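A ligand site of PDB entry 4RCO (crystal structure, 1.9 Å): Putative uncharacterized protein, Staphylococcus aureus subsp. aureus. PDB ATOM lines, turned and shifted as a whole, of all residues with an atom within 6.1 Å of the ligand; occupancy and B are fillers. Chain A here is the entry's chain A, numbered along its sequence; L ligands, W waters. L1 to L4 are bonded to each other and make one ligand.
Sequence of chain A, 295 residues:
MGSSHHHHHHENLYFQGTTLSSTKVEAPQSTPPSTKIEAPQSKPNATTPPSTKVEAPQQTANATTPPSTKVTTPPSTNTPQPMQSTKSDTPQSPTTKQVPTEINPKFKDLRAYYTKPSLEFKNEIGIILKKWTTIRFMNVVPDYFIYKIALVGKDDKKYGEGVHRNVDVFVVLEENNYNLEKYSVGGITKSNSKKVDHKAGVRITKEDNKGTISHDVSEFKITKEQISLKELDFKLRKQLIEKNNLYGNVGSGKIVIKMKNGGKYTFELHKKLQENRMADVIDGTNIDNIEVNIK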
ATOM      1  N   LYS A 154      21.277  30.942 -21.943  1.00  0.00           N
ATOM      2  CA  LYS A 154      22.150  32.039 -22.413  1.00  0.00           C
ATOM      3  C   LYS A 154      22.758  31.803 -23.781  1.00  0.00           C
ATOM      4  O   LYS A 154      23.190  32.736 -24.419  1.00  0.00           O
ATOM      5  CB  LYS A 154      23.270  32.292 -21.405  1.00  0.00           C
ATOM      6  CG  LYS A 154      22.782  32.789 -20.052  1.00  0.00           C
ATOM      7  CD  LYS A 154      23.945  32.960 -19.090  1.00  0.00           C
ATOM      8  CE  LYS A 154      23.496  33.429 -17.713  1.00  0.00           C
ATOM      9  NZ  LYS A 154      22.650  32.431 -17.002  1.00  0.00           N
ATOM     10  N   LEU A 229      27.893  23.565 -16.764  1.00  0.00           N
ATOM     11  CA  LEU A 229      27.196  22.908 -15.674  1.00  0.00           C
ATOM     12  C   LEU A 229      26.640  21.579 -16.192  1.00  0.00           C
ATOM     13  O   LEU A 229      26.522  20.641 -15.432  1.00  0.00           O
ATOM     14  CB  LEU A 229      26.061  23.759 -15.095  1.00  0.00           C
ATOM     15  CG  LEU A 229      26.471  25.099 -14.497  1.00  0.00           C
ATOM     16  CD1 LEU A 229      25.256  25.713 -13.840  1.00  0.00           C
ATOM     17  CD2 LEU A 229      27.583  24.955 -13.455  1.00  0.00           C
ATOM     18  N   MET A 259      33.299  27.485  -5.357  1.00  0.00           N
ATOM     19  CA  MET A 259      34.336  28.166  -6.132  1.00  0.00           C
ATOM     20  C   MET A 259      35.334  28.863  -5.221  1.00  0.00           C
ATOM     21  O   MET A 259      35.008  29.200  -4.092  1.00  0.00           O
ATOM     22  CB  MET A 259      33.693  29.203  -7.035  1.00  0.00           C
ATOM     23  CG  MET A 259      32.556  28.618  -7.885  1.00  0.00           C
ATOM     24  SD  MET A 259      33.074  27.259  -8.945  1.00  0.00           S
ATOM     25  CE  MET A 259      34.017  28.222 -10.113  1.00  0.00           C
ATOM     26  N   GLY A 263      31.785  31.600  -4.575  1.00  0.00           N
ATOM     27  CA  GLY A 263      30.576  31.276  -5.325  1.00  0.00           C
ATOM     28  C   GLY A 263      30.217  29.800  -5.208  1.00  0.00           C
ATOM     29  O   GLY A 263      31.056  29.002  -4.777  1.00  0.00           O
ATOM     30  N   LYS A 264      28.986  29.455  -5.568  1.00  0.00           N
ATOM     31  CA  LYS A 264      28.517  28.052  -5.541  1.00  0.00           C
ATOM     32  C   LYS A 264      27.543  27.818  -6.678  1.00  0.00           C
ATOM     33  O   LYS A 264      26.894  28.760  -7.105  1.00  0.00           O
ATOM     34  CB  LYS A 264      27.810  27.727  -4.225  1.00  0.00           C
ATOM     35  CG  LYS A 264      26.458  28.364  -4.087  1.00  0.00           C
ATOM     36  CD  LYS A 264      25.907  28.230  -2.689  1.00  0.00           C
ATOM     37  CE  LYS A 264      24.470  28.752  -2.628  1.00  0.00           C
ATOM     38  NZ  LYS A 264      23.846  28.480  -1.297  1.00  0.00           N
ATOM     39  N   TYR A 265      27.408  26.554  -7.094  1.00  0.00           N
ATOM     40  CA  TYR A 265      26.479  26.117  -8.115  1.00  0.00           C
ATOM     41  C   TYR A 265      25.860  24.855  -7.535  1.00  0.00           C
ATOM     42  O   TYR A 265      26.564  23.952  -7.152  1.00  0.00           O
ATOM     43  CB  TYR A 265      27.176  25.852  -9.466  1.00  0.00           C
ATOM     44  CG  TYR A 265      27.809  27.102 -10.013  1.00  0.00           C
ATOM     45  CD1 TYR A 265      27.068  28.008 -10.747  1.00  0.00           C
ATOM     46  CD2 TYR A 265      29.153  27.422  -9.738  1.00  0.00           C
ATOM     47  CE1 TYR A 265      27.620  29.195 -11.193  1.00  0.00           C
ATOM     48  CE2 TYR A 265      29.706  28.608 -10.206  1.00  0.00           C
ATOM     49  CZ  TYR A 265      28.949  29.467 -10.931  1.00  0.00           C
ATOM     50  OH  TYR A 265      29.506  30.632 -11.372  1.00  0.00           O
ATOM     51  N   THR A 266      24.530  24.812  -7.462  1.00  0.00           N
ATOM     52  CA  THR A 266      23.852  23.685  -6.851  1.00  0.00           C
ATOM     53  C   THR A 266      23.052  22.832  -7.819  1.00  0.00           C
ATOM     54  O   THR A 266      22.298  23.342  -8.636  1.00  0.00           O
ATOM     55  CB  THR A 266      22.901  24.216  -5.781  1.00  0.00           C
ATOM     56  OG1 THR A 266      23.662  24.984  -4.835  1.00  0.00           O
ATOM     57  CG2 THR A 266      22.168  23.081  -5.096  1.00  0.00           C
ATOM     58  N   PHE A 267      23.210  21.512  -7.697  1.00  0.00           N
ATOM     59  CA  PHE A 267      22.438  20.563  -8.502  1.00  0.00           C
ATOM     60  C   PHE A 267      21.577  19.734  -7.535  1.00  0.00           C
ATOM     61  O   PHE A 267      22.108  18.996  -6.695  1.00  0.00           O
ATOM     62  CB  PHE A 267      23.304  19.623  -9.361  1.00  0.00           C
ATOM     63  CG  PHE A 267      24.398  20.312 -10.152  1.00  0.00           C
ATOM     64  CD1 PHE A 267      24.153  21.460 -10.892  1.00  0.00           C
ATOM     65  CD2 PHE A 267      25.673  19.732 -10.234  1.00  0.00           C
ATOM     66  CE1 PHE A 267      25.176  22.083 -11.621  1.00  0.00           C
ATOM     67  CE2 PHE A 267      26.687  20.326 -10.977  1.00  0.00           C
ATOM     68  CZ  PHE A 267      26.431  21.498 -11.668  1.00  0.00           C
ATOM     69  N   GLU A 268      20.247  19.873  -7.643  1.00  0.00           N
ATOM     70  CA  GLU A 268      19.321  19.150  -6.770  1.00  0.00           C
ATOM     71  C   GLU A 268      19.178  17.753  -7.368  1.00  0.00           C
ATOM     72  O   GLU A 268      18.778  17.610  -8.542  1.00  0.00           O
ATOM     73  CB  GLU A 268      17.952  19.841  -6.728  1.00  0.00           C
ATOM     74  CG  GLU A 268      18.010  21.275  -6.237  1.00  0.00           C
ATOM     75  CD  GLU A 268      16.645  21.955  -6.249  1.00  0.00           C
ATOM     76  OE1 GLU A 268      16.313  22.587  -7.256  1.00  0.00           O
ATOM     77  OE2 GLU A 268      15.903  21.765  -5.299  1.00  0.00           O
ATOM     78  N   HIS A 270      17.085  15.167  -6.826  1.00  0.00           N
ATOM     79  CA  HIS A 270      15.785  14.532  -7.005  1.00  0.00           C
ATOM     80  C   HIS A 270      15.139  14.727  -8.363  1.00  0.00           C
ATOM     81  O   HIS A 270      14.071  14.134  -8.629  1.00  0.00           O
ATOM     82  CB  HIS A 270      14.815  14.976  -5.912  1.00  0.00           C
ATOM     83  CG  HIS A 270      14.375  16.387  -6.059  1.00  0.00           C
ATOM     84  ND1 HIS A 270      15.140  17.456  -5.637  1.00  0.00           N
ATOM     85  CD2 HIS A 270      13.249  16.918  -6.597  1.00  0.00           C
ATOM     86  CE1 HIS A 270      14.502  18.581  -5.910  1.00  0.00           C
ATOM     87  NE2 HIS A 270      13.351  18.278  -6.484  1.00  0.00           N
ATOM     88  N   LYS A 271      15.729  15.594  -9.205  1.00  0.00           N
ATOM     89  CA  LYS A 271      15.245  15.857 -10.577  1.00  0.00           C
ATOM     90  C   LYS A 271      16.400  16.183 -11.507  1.00  0.00           C
ATOM     91  O   LYS A 271      17.492  16.487 -11.056  1.00  0.00           O
ATOM     92  CB  LYS A 271      14.248  17.020 -10.590  1.00  0.00           C
ATOM     93  CG  LYS A 271      14.798  18.349 -10.143  1.00  0.00           C
ATOM     94  CD  LYS A 271      13.699  19.383  -9.956  1.00  0.00           C
ATOM     95  CE  LYS A 271      14.243  20.734  -9.470  1.00  0.00           C
ATOM     96  NZ  LYS A 271      13.182  21.760  -9.272  1.00  0.00           N
ATOM     97  N   GLN A 274      17.990  21.495 -14.727  1.00  0.00           N
ATOM     98  CA  GLN A 274      17.079  22.273 -15.558  1.00  0.00           C
ATOM     99  C   GLN A 274      17.755  22.554 -16.897  1.00  0.00           C
ATOM    100  O   GLN A 274      18.928  22.989 -16.943  1.00  0.00           O
ATOM    101  CB  GLN A 274      16.643  23.570 -14.857  1.00  0.00           C
ATOM    102  CG  GLN A 274      16.025  23.348 -13.495  1.00  0.00           C
ATOM    103  CD  GLN A 274      17.014  23.487 -12.337  1.00  0.00           C
ATOM    104  OE1 GLN A 274      18.130  23.003 -12.391  1.00  0.00           O
ATOM    105  NE2 GLN A 274      16.584  24.163 -11.271  1.00  0.00           N
ATOM    106  N   GLU A 275      17.019  22.392 -17.997  1.00  0.00           N
ATOM    107  CA  GLU A 275      17.672  22.546 -19.321  1.00  0.00           C
ATOM    108  C   GLU A 275      18.437  23.842 -19.565  1.00  0.00           C
ATOM    109  O   GLU A 275      19.537  23.816 -20.151  1.00  0.00           O
ATOM    110  CB  GLU A 275      16.713  22.267 -20.501  1.00  0.00           C
ATOM    111  CG  GLU A 275      16.538  20.778 -20.763  1.00  0.00           C
ATOM    112  CD  GLU A 275      15.928  20.474 -22.120  1.00  0.00           C
ATOM    113  OE1 GLU A 275      15.551  21.416 -22.847  1.00  0.00           O
ATOM    114  OE2 GLU A 275      15.871  19.307 -22.472  1.00  0.00           O
ATOM    115  N   ASN A 276      17.864  24.961 -19.165  1.00  0.00           N
ATOM    116  CA  ASN A 276      18.508  26.232 -19.368  1.00  0.00           C
ATOM    117  C   ASN A 276      19.893  26.271 -18.728  1.00  0.00           C
ATOM    118  O   ASN A 276      20.828  26.833 -19.280  1.00  0.00           O
ATOM    119  CB  ASN A 276      17.625  27.407 -18.912  1.00  0.00           C
ATOM    120  CG  ASN A 276      17.433  27.434 -17.388  1.00  0.00           C
ATOM    121  OD1 ASN A 276      16.790  26.554 -16.811  1.00  0.00           O
ATOM    122  ND2 ASN A 276      17.974  28.450 -16.748  1.00  0.00           N
ATOM    123  N   ARG A 277      20.052  25.626 -17.561  1.00  0.00           N
ATOM    124  CA  ARG A 277      21.322  25.629 -16.876  1.00  0.00           C
ATOM    125  C   ARG A 277      22.380  24.742 -17.559  1.00  0.00           C
ATOM    126  O   ARG A 277      23.565  24.840 -17.249  1.00  0.00           O
ATOM    127  CB  ARG A 277      21.148  25.211 -15.424  1.00  0.00           C
ATOM    128  CG  ARG A 277      20.131  26.080 -14.694  1.00  0.00           C
ATOM    129  CD  ARG A 277      19.965  25.609 -13.277  1.00  0.00           C
ATOM    130  NE  ARG A 277      21.182  25.696 -12.505  1.00  0.00           N
ATOM    131  CZ  ARG A 277      21.480  24.958 -11.435  1.00  0.00           C
ATOM    132  NH1 ARG A 277      20.719  23.939 -11.052  1.00  0.00           N
ATOM    133  NH2 ARG A 277      22.612  25.184 -10.793  1.00  0.00           N
ATOM    134  N   ASP A 280      24.811  27.071 -18.971  1.00  0.00           N
ATOM    135  CA  ASP A 280      25.628  27.919 -18.096  1.00  0.00           C
ATOM    136  C   ASP A 280      27.051  27.351 -18.044  1.00  0.00           C
ATOM    137  O   ASP A 280      27.257  26.131 -18.011  1.00  0.00           O
ATOM    138  CB  ASP A 280      25.022  28.002 -16.685  1.00  0.00           C
ATOM    139  CG  ASP A 280      23.790  28.838 -16.646  1.00  0.00           C
ATOM    140  OD1 ASP A 280      23.720  29.815 -17.453  1.00  0.00           O
ATOM    141  OD2 ASP A 280      22.881  28.539 -15.816  1.00  0.00           O
HETATM  142  C1  LIG L   1      22.852  27.884  -7.002  1.00  0.00           C
HETATM  143  C2  LIG L   1      22.220  29.221  -7.333  1.00  0.00           C
HETATM  144  C3  LIG L   1      22.687  30.298  -6.330  1.00  0.00           C
HETATM  145  C4  LIG L   1      24.129  30.755  -6.577  1.00  0.00           C
HETATM  146  C5  LIG L   1      24.417  31.087  -8.037  1.00  0.00           C
HETATM  147  C6  LIG L   1      23.896  29.911  -8.897  1.00  0.00           C
HETATM  148  C7  LIG L   1      23.962  30.136 -10.394  1.00  0.00           C
HETATM  149  C8  LIG L   1      23.227  29.007 -11.123  1.00  0.00           C
HETATM  150  C9  LIG L   1      23.513  28.981 -12.608  1.00  0.00           C
HETATM  151  C10 LIG L   1      26.418  32.373  -8.604  1.00  0.00           C
HETATM  152  C11 LIG L   1      27.927  32.398  -8.694  1.00  0.00           C
HETATM  153  N1  LIG L   1      25.861  31.249  -8.168  1.00  0.00           N
HETATM  154  O1  LIG L   1      23.176  27.120  -7.931  1.00  0.00           O
HETATM  155  O2  LIG L   1      23.054  27.578  -5.786  1.00  0.00           O
HETATM  156  O3  LIG L   1      24.361  31.901  -5.753  1.00  0.00           O
HETATM  157  O4  LIG L   1      22.526  29.735  -8.612  1.00  0.00           O
HETATM  158  O5  LIG L   1      23.385  31.411 -10.722  1.00  0.00           O
HETATM  159  O6  LIG L   1      23.623  27.732 -10.595  1.00  0.00           O
HETATM  160  O7  LIG L   1      22.779  27.954 -13.280  1.00  0.00           O
HETATM  161  O8  LIG L   1      25.750  33.329  -8.929  1.00  0.00           O
HETATM  162  C1  LG2 L   2      18.463  27.859  -9.763  1.00  0.00           C
HETATM  163  C2  LG2 L   2      19.054  28.888  -8.791  1.00  0.00           C
HETATM  164  C3  LG2 L   2      20.252  28.313  -8.106  1.00  0.00           C
HETATM  165  C4  LG2 L   2      19.876  26.968  -7.513  1.00  0.00           C
HETATM  166  C5  LG2 L   2      19.180  26.043  -8.508  1.00  0.00           C
HETATM  167  C6  LG2 L   2      18.656  24.771  -7.831  1.00  0.00           C
HETATM  168  O1  LG2 L   2      19.374  30.029  -9.525  1.00  0.00           O
HETATM  169  O2  LG2 L   2      20.784  29.203  -7.102  1.00  0.00           O
HETATM  170  O3  LG2 L   2      19.010  27.216  -6.408  1.00  0.00           O
HETATM  171  O4  LG2 L   2      18.096  26.697  -9.096  1.00  0.00           O
HETATM  172  O5  LG2 L   2      18.098  23.877  -8.791  1.00  0.00           O
HETATM  173  C1  LG3 L   3      15.554  28.402 -14.029  1.00  0.00           C
HETATM  174  C2  LG3 L   3      15.020  27.422 -12.995  1.00  0.00           C
HETATM  175  C3  LG3 L   3      15.436  27.850 -11.620  1.00  0.00           C
HETATM  176  C4  LG3 L   3      16.932  28.073 -11.571  1.00  0.00           C
HETATM  177  C5  LG3 L   3      17.332  29.092 -12.578  1.00  0.00           C
HETATM  178  C6  LG3 L   3      18.838  29.353 -12.596  1.00  0.00           C
HETATM  179  C7  LG3 L   3      12.931  26.347 -13.675  1.00  0.00           C
HETATM  180  C8  LG3 L   3      11.427  26.330 -13.675  1.00  0.00           C
HETATM  181  O1  LG3 L   3      16.957  28.596 -13.844  1.00  0.00           O
HETATM  182  O2  LG3 L   3      15.102  26.816 -10.735  1.00  0.00           O
HETATM  183  O3  LG3 L   3      17.314  28.497 -10.281  1.00  0.00           O
HETATM  184  O4  LG3 L   3      19.071  30.295 -13.626  1.00  0.00           O
HETATM  185  O5  LG3 L   3      13.587  25.485 -14.234  1.00  0.00           O
HETATM  186  N1  LG3 L   3      13.558  27.375 -13.060  1.00  0.00           N
HETATM  187  O6  LG3 L   3      14.874  29.643 -13.849  1.00  0.00           O
HETATM  188  C1  LG4 L   4      13.905  27.018  -9.972  1.00  0.00           C
HETATM  189  C2  LG4 L   4      13.553  25.637  -9.396  1.00  0.00           C
HETATM  190  C3  LG4 L   4      14.518  25.197  -8.305  1.00  0.00           C
HETATM  191  C4  LG4 L   4      14.638  26.288  -7.237  1.00  0.00           C
HETATM  192  C5  LG4 L   4      15.014  27.591  -7.950  1.00  0.00           C
HETATM  193  C6  LG4 L   4      15.186  28.720  -6.940  1.00  0.00           C
HETATM  194  O1  LG4 L   4      13.599  24.685 -10.438  1.00  0.00           O
HETATM  195  O2  LG4 L   4      14.143  23.965  -7.713  1.00  0.00           O
HETATM  196  O3  LG4 L   4      13.427  26.401  -6.482  1.00  0.00           O
HETATM  197  O4  LG4 L   4      14.060  27.988  -8.951  1.00  0.00           O
HETATM  198  O   HOH W   1      14.844  30.574 -16.270  1.00  0.00           O
HETATM  199  O   HOH W   2      18.890  25.278  -4.512  1.00  0.00           O
HETATM  200  O   HOH W   3      25.267  32.909 -11.958  1.00  0.00           O
HETATM  201  O   HOH W   4      19.420  21.581  -9.764  1.00  0.00           O
HETATM  202  O   HOH W   5      20.124  32.761 -12.552  1.00  0.00           O
HETATM  203  O   HOH W   6      11.862  24.327  -5.905  1.00  0.00           O
HETATM  204  O   HOH W   7      17.326  32.186 -14.947  1.00  0.00           O
HETATM  205  O   HOH W   8      14.359  30.687  -9.696  1.00  0.00           O
HETATM  206  O   HOH W   9      13.102  23.485 -15.861  1.00  0.00           O
HETATM  207  O   HOH W  10      14.443  26.649  -4.162  1.00  0.00           O
HETATM  208  O   HOH W  11      17.057  31.697  -9.653  1.00  0.00           O
HETATM  209  O   HOH W  12      20.997  28.118  -3.939  1.00  0.00           O
HETATM  210  O   HOH W  13      18.495  29.682  -5.006  1.00  0.00           O
HETATM  211  O   HOH W  14      20.922  30.260 -15.395  1.00  0.00           O
HETATM  212  O   HOH W  15      21.127  32.250  -9.758  1.00  0.00           O
HETATM  213  O   HOH W  16      22.665  32.551  -3.614  1.00  0.00           O
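OD2 of Asp 280 is in hydrogen-bond range of O7 of LIG L1 (2.6 Å). The side-chain carboxylate (OE1) of Glu 268 sits at hydrogen-bond distance from an oxygen (O2) of LG4 L4 (2.6 Å). O1 of LIG L1 sits at hydrogen-bond distance from N of Thr 266. The side-chain hydroxyl (OG1) of Thr 266 sits at hydrogen-bond distance from an oxygen (O2) of LIG L1 (2.8 Å). O1 of LIG L1 is in salt-bridge range of NH2 of Arg 277 (3.5 Å). The side-chain amino group (NZ) of Lys 271 sits at hydrogen-bond distance from an oxygen (O2) of LG4 L4 (2.9 Å). The backbone carbonyl oxygen (O) of Lys 264 sits at hydrogen-bond distance from a nitrogen (N1) of LIG L1, 2.9 Å away. NE2 of Gln 274 lies within hydrogen-bond range of O5 of LG2 L2, 2.9 Å away. An oxygen (O1) of LG3 L3 sits at hydrogen-bond distance from the side-chain amide nitrogen (ND2) of Asn 276, at 3.1 Å.
N of Leu 229 sits at hydrogen-bond distance from O of Asp 280 (2.9 Å). The side-chain amino group of Lys 154 is in salt-bridge range of the side-chain carboxylate of Asp 280 (2.9 Å). The side-chain carboxylate (OE1) of Glu 268 is in salt-bridge range of the side-chain amino group (NZ) of Lys 271, 3.8 Å away. The backbone carbonyl oxygen (O) of Thr 266 is in hydrogen-bond range of the guanidinium group (NH2) of Arg 277, at 2.9 Å. The side-chain amide oxygen of Gln 274 sits at hydrogen-bond distance from the guanidinium group of Arg 277 (3.1 Å).
Residues that only touch the ligand: Leu 229 and Tyr 265. Hydrophobic or aromatic side chains that line the ligand: Leu 229 and Tyr 265. Of the 16 residues printed, 10 come within 4 Å of the ligand. The nearest printed residue that does not touch the ligand is Gly 263 (4.4 Å).
Water W14 lies within hydrogen-bond range of an oxygen (O4) of LG3 L3 (2.6 Å), the side-chain carboxylate (OD2) of Asp 280 (2.6 Å) and the side-chain amino group (NZ) of Lys 154 (3.2 Å). Water W4 lies within hydrogen-bond range of O5 of LG2 L2, N of Glu 268, NH1 of Arg 277 and OE1 of Gln 274.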
